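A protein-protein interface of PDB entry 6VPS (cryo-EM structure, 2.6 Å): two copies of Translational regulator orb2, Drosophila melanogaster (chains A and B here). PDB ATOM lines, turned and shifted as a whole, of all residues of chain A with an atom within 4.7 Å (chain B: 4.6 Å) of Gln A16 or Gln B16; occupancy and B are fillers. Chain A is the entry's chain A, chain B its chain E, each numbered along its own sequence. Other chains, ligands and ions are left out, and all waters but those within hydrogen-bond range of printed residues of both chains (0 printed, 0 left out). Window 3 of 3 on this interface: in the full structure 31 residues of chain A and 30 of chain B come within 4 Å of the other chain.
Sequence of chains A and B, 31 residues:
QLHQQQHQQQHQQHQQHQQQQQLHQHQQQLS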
ATOM      1  N   HIS A  14      26.669 -12.096 -17.751  1.00  0.00           N
ATOM      2  CA  HIS A  14      26.145 -12.122 -19.123  1.00  0.00           C
ATOM      3  C   HIS A  14      26.631 -13.374 -19.840  1.00  0.00           C
ATOM      4  O   HIS A  14      27.515 -13.299 -20.703  1.00  0.00           O
ATOM      5  CB  HIS A  14      26.500 -10.807 -19.871  1.00  0.00           C
ATOM      6  CG  HIS A  14      25.659 -10.541 -21.074  1.00  0.00           C
ATOM      7  ND1 HIS A  14      24.292 -10.328 -20.990  1.00  0.00           N
ATOM      8  CD2 HIS A  14      25.986 -10.390 -22.379  1.00  0.00           C
ATOM      9  CE1 HIS A  14      23.810 -10.113 -22.199  1.00  0.00           C
ATOM     10  NE2 HIS A  14      24.827 -10.144 -23.068  1.00  0.00           N
ATOM     11  N   GLN A  15      26.071 -14.526 -19.433  1.00  0.00           N
ATOM     12  CA  GLN A  15      26.537 -15.830 -19.876  1.00  0.00           C
ATOM     13  C   GLN A  15      25.370 -16.748 -20.116  1.00  0.00           C
ATOM     14  O   GLN A  15      24.300 -16.562 -19.539  1.00  0.00           O
ATOM     15  CB  GLN A  15      27.526 -16.420 -18.876  1.00  0.00           C
ATOM     16  CG  GLN A  15      27.020 -16.472 -17.446  1.00  0.00           C
ATOM     17  CD  GLN A  15      27.980 -17.200 -16.536  1.00  0.00           C
ATOM     18  OE1 GLN A  15      29.134 -17.461 -16.884  1.00  0.00           O
ATOM     19  NE2 GLN A  15      27.503 -17.563 -15.359  1.00  0.00           N
ATOM     20  N   GLN A  16      25.651 -17.838 -20.820  1.00  0.00           N
ATOM     21  CA  GLN A  16      24.639 -18.754 -21.297  1.00  0.00           C
ATOM     22  C   GLN A  16      25.325 -20.086 -21.586  1.00  0.00           C
ATOM     23  O   GLN A  16      26.398 -20.098 -22.186  1.00  0.00           O
ATOM     24  CB  GLN A  16      24.082 -18.145 -22.576  1.00  0.00           C
ATOM     25  CG  GLN A  16      22.718 -18.616 -22.972  1.00  0.00           C
ATOM     26  CD  GLN A  16      22.431 -18.180 -24.385  1.00  0.00           C
ATOM     27  OE1 GLN A  16      23.315 -18.151 -25.242  1.00  0.00           O
ATOM     28  NE2 GLN A  16      21.191 -17.821 -24.640  1.00  0.00           N
ATOM     29  N   HIS A  17      24.713 -21.197 -21.120  1.00  0.00           N
ATOM     30  CA  HIS A  17      25.174 -22.574 -21.382  1.00  0.00           C
ATOM     31  C   HIS A  17      26.478 -22.877 -20.651  1.00  0.00           C
ATOM     32  O   HIS A  17      27.543 -23.032 -21.280  1.00  0.00           O
ATOM     33  CB  HIS A  17      25.269 -22.872 -22.892  1.00  0.00           C
ATOM     34  CG  HIS A  17      24.021 -22.569 -23.633  1.00  0.00           C
ATOM     35  ND1 HIS A  17      22.818 -23.220 -23.359  1.00  0.00           N
ATOM     36  CD2 HIS A  17      23.760 -21.671 -24.605  1.00  0.00           C
ATOM     37  CE1 HIS A  17      21.881 -22.717 -24.119  1.00  0.00           C
ATOM     38  NE2 HIS A  17      22.438 -21.774 -24.903  1.00  0.00           N
ATOM     39  N   GLN A  18      26.392 -22.965 -19.328  1.00  0.00           N
ATOM     40  CA  GLN A  18      27.522 -23.385 -18.515  1.00  0.00           C
ATOM     41  C   GLN A  18      27.072 -24.554 -17.674  1.00  0.00           C
ATOM     42  O   GLN A  18      27.265 -24.552 -16.458  1.00  0.00           O
ATOM     43  CB  GLN A  18      27.979 -22.256 -17.577  1.00  0.00           C
ATOM     44  CG  GLN A  18      28.841 -21.190 -18.225  1.00  0.00           C
ATOM     45  CD  GLN A  18      28.001 -20.166 -18.913  1.00  0.00           C
ATOM     46  OE1 GLN A  18      26.876 -19.881 -18.506  1.00  0.00           O
ATOM     47  NE2 GLN A  18      28.511 -19.646 -20.009  1.00  0.00           N
ATOM     48  N   GLN B  15      22.247 -14.505 -16.584  1.00  0.00           N
ATOM     49  CA  GLN B  15      22.693 -15.809 -17.055  1.00  0.00           C
ATOM     50  C   GLN B  15      21.506 -16.696 -17.336  1.00  0.00           C
ATOM     51  O   GLN B  15      20.428 -16.467 -16.813  1.00  0.00           O
ATOM     52  CB  GLN B  15      23.641 -16.445 -16.045  1.00  0.00           C
ATOM     53  CG  GLN B  15      23.127 -16.439 -14.627  1.00  0.00           C
ATOM     54  CD  GLN B  15      23.986 -17.266 -13.697  1.00  0.00           C
ATOM     55  OE1 GLN B  15      25.141 -17.568 -13.980  1.00  0.00           O
ATOM     56  NE2 GLN B  15      23.405 -17.667 -12.579  1.00  0.00           N
ATOM     57  N   GLN B  16      21.782 -17.818 -17.998  1.00  0.00           N
ATOM     58  CA  GLN B  16      20.764 -18.706 -18.511  1.00  0.00           C
ATOM     59  C   GLN B  16      21.435 -20.038 -18.844  1.00  0.00           C
ATOM     60  O   GLN B  16      22.490 -20.051 -19.470  1.00  0.00           O
ATOM     61  CB  GLN B  16      20.258 -18.064 -19.787  1.00  0.00           C
ATOM     62  CG  GLN B  16      18.876 -18.444 -20.177  1.00  0.00           C
ATOM     63  CD  GLN B  16      18.605 -17.991 -21.583  1.00  0.00           C
ATOM     64  OE1 GLN B  16      19.506 -17.919 -22.423  1.00  0.00           O
ATOM     65  NE2 GLN B  16      17.344 -17.736 -21.874  1.00  0.00           N
ATOM     66  N   HIS B  17      20.805 -21.149 -18.423  1.00  0.00           N
ATOM     67  CA  HIS B  17      21.249 -22.529 -18.692  1.00  0.00           C
ATOM     68  C   HIS B  17      22.549 -22.854 -17.973  1.00  0.00           C
ATOM     69  O   HIS B  17      23.601 -23.035 -18.613  1.00  0.00           O
ATOM     70  CB  HIS B  17      21.360 -22.807 -20.184  1.00  0.00           C
ATOM     71  CG  HIS B  17      20.135 -22.467 -20.933  1.00  0.00           C
ATOM     72  ND1 HIS B  17      18.940 -23.123 -20.716  1.00  0.00           N
ATOM     73  CD2 HIS B  17      19.896 -21.516 -21.859  1.00  0.00           C
ATOM     74  CE1 HIS B  17      18.021 -22.570 -21.443  1.00  0.00           C
ATOM     75  NE2 HIS B  17      18.592 -21.606 -22.188  1.00  0.00           N
ATOM     76  N   GLN B  18      22.469 -22.957 -16.657  1.00  0.00           N
ATOM     77  CA  GLN B  18      23.596 -23.421 -15.865  1.00  0.00           C
ATOM     78  C   GLN B  18      23.123 -24.604 -15.053  1.00  0.00           C
ATOM     79  O   GLN B  18      23.353 -24.661 -13.843  1.00  0.00           O
ATOM     80  CB  GLN B  18      24.112 -22.315 -14.932  1.00  0.00           C
ATOM     81  CG  GLN B  18      24.924 -21.216 -15.616  1.00  0.00           C
ATOM     82  CD  GLN B  18      24.037 -20.178 -16.228  1.00  0.00           C
ATOM     83  OE1 GLN B  18      22.946 -19.882 -15.728  1.00  0.00           O
ATOM     84  NE2 GLN B  18      24.471 -19.641 -17.348  1.00  0.00           N
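Hydrophobic or aromatic side chains of chain B within 4 Å of the printed part of chain A: His B17. Among the printed residues, no Asp or Glu carboxylate lies within 4 Å of a Lys or Arg side-chain nitrogen of the other chain.
OE1 of Gln A18 lies within hydrogen-bond range of NE2 of Gln B18, 2.7 Å away. O of His B17 lies within hydrogen-bond range of N of Gln A18, 2.9 Å away. The backbone carbonyl oxygen (O) of Gln A15 lies within hydrogen-bond range of the backbone NH (N) of Gln B16. N of His A17 is in hydrogen-bond range of O of Gln B16 (3.0 Å). The side-chain amide nitrogen (NE2) of Gln A16 sits at hydrogen-bond distance from the side-chain amide oxygen (OE1) of Gln B16 (2.8 Å). The side-chain amide oxygen (OE1) of Gln B15 sits at hydrogen-bond distance from the side-chain amide nitrogen (NE2) of Gln A15, 2.7 Å away. The backbone NH of His A17 sits close to the backbone carbonyl oxygen of His B17, 3.3 Å away.
The side-chain amide nitrogen (NE2) of Gln A18 sits at hydrogen-bond distance from the backbone carbonyl oxygen (O) of Gln A16, at 3.1 Å. NE2 of Gln B18 is in hydrogen-bond range of O of Gln B16 (2.9 Å).
Gln A15 touches Gln B16, but with the chains exchanged Gln A16 does not touch Gln B15 (5.2 Å). Gln A15 touches Gln B18, but with the chains exchanged Gln A18 does not touch Gln B15 (5.3 Å). His A17 touches Gln B16, but with the chains exchanged Gln A16 does not touch His B17 (4.2 Å). Gln B18 touches its own counterpart, Gln A18. 4 positions are printed for both chains. Of the 8 pairs that touch across the chains among the printed residues, 4 have their exchanged pair printed and touching as well.
Gln A16 touches just one residue of chain B: Gln B16 (2.8 Å). Of chain A, only Gln A15 (3.2 Å), Gln A16 (2.8 Å) and His A17 (3.0 Å) come within 4 Å of Gln B16. Of the printed residues of chain B, Gln A15 touches Gln B15 (2.7 Å), Gln B16 (3.2 Å) and Gln B18 (3.8 Å). Printed residues of chain A within 4 Å of Gln B18: Gln A15 (3.8 Å) and Gln A18 (2.7 Å). Printed residues of chain B within 4 Å of Gln A18: His B17 and Gln B18. Of the printed residues of chain A, His B17 touches His A17 and Gln A18. The nearest residue of chain A that does not touch Gln B16 is Gln A18 (4.5 Å). The nearest printed residue of chain B that does not touch Gln A18 is Gln B16 (4.5 Å).
Among the printed residues, pairs that only touch across the chains: Gln A15 with Gln B18 (3.8 Å).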
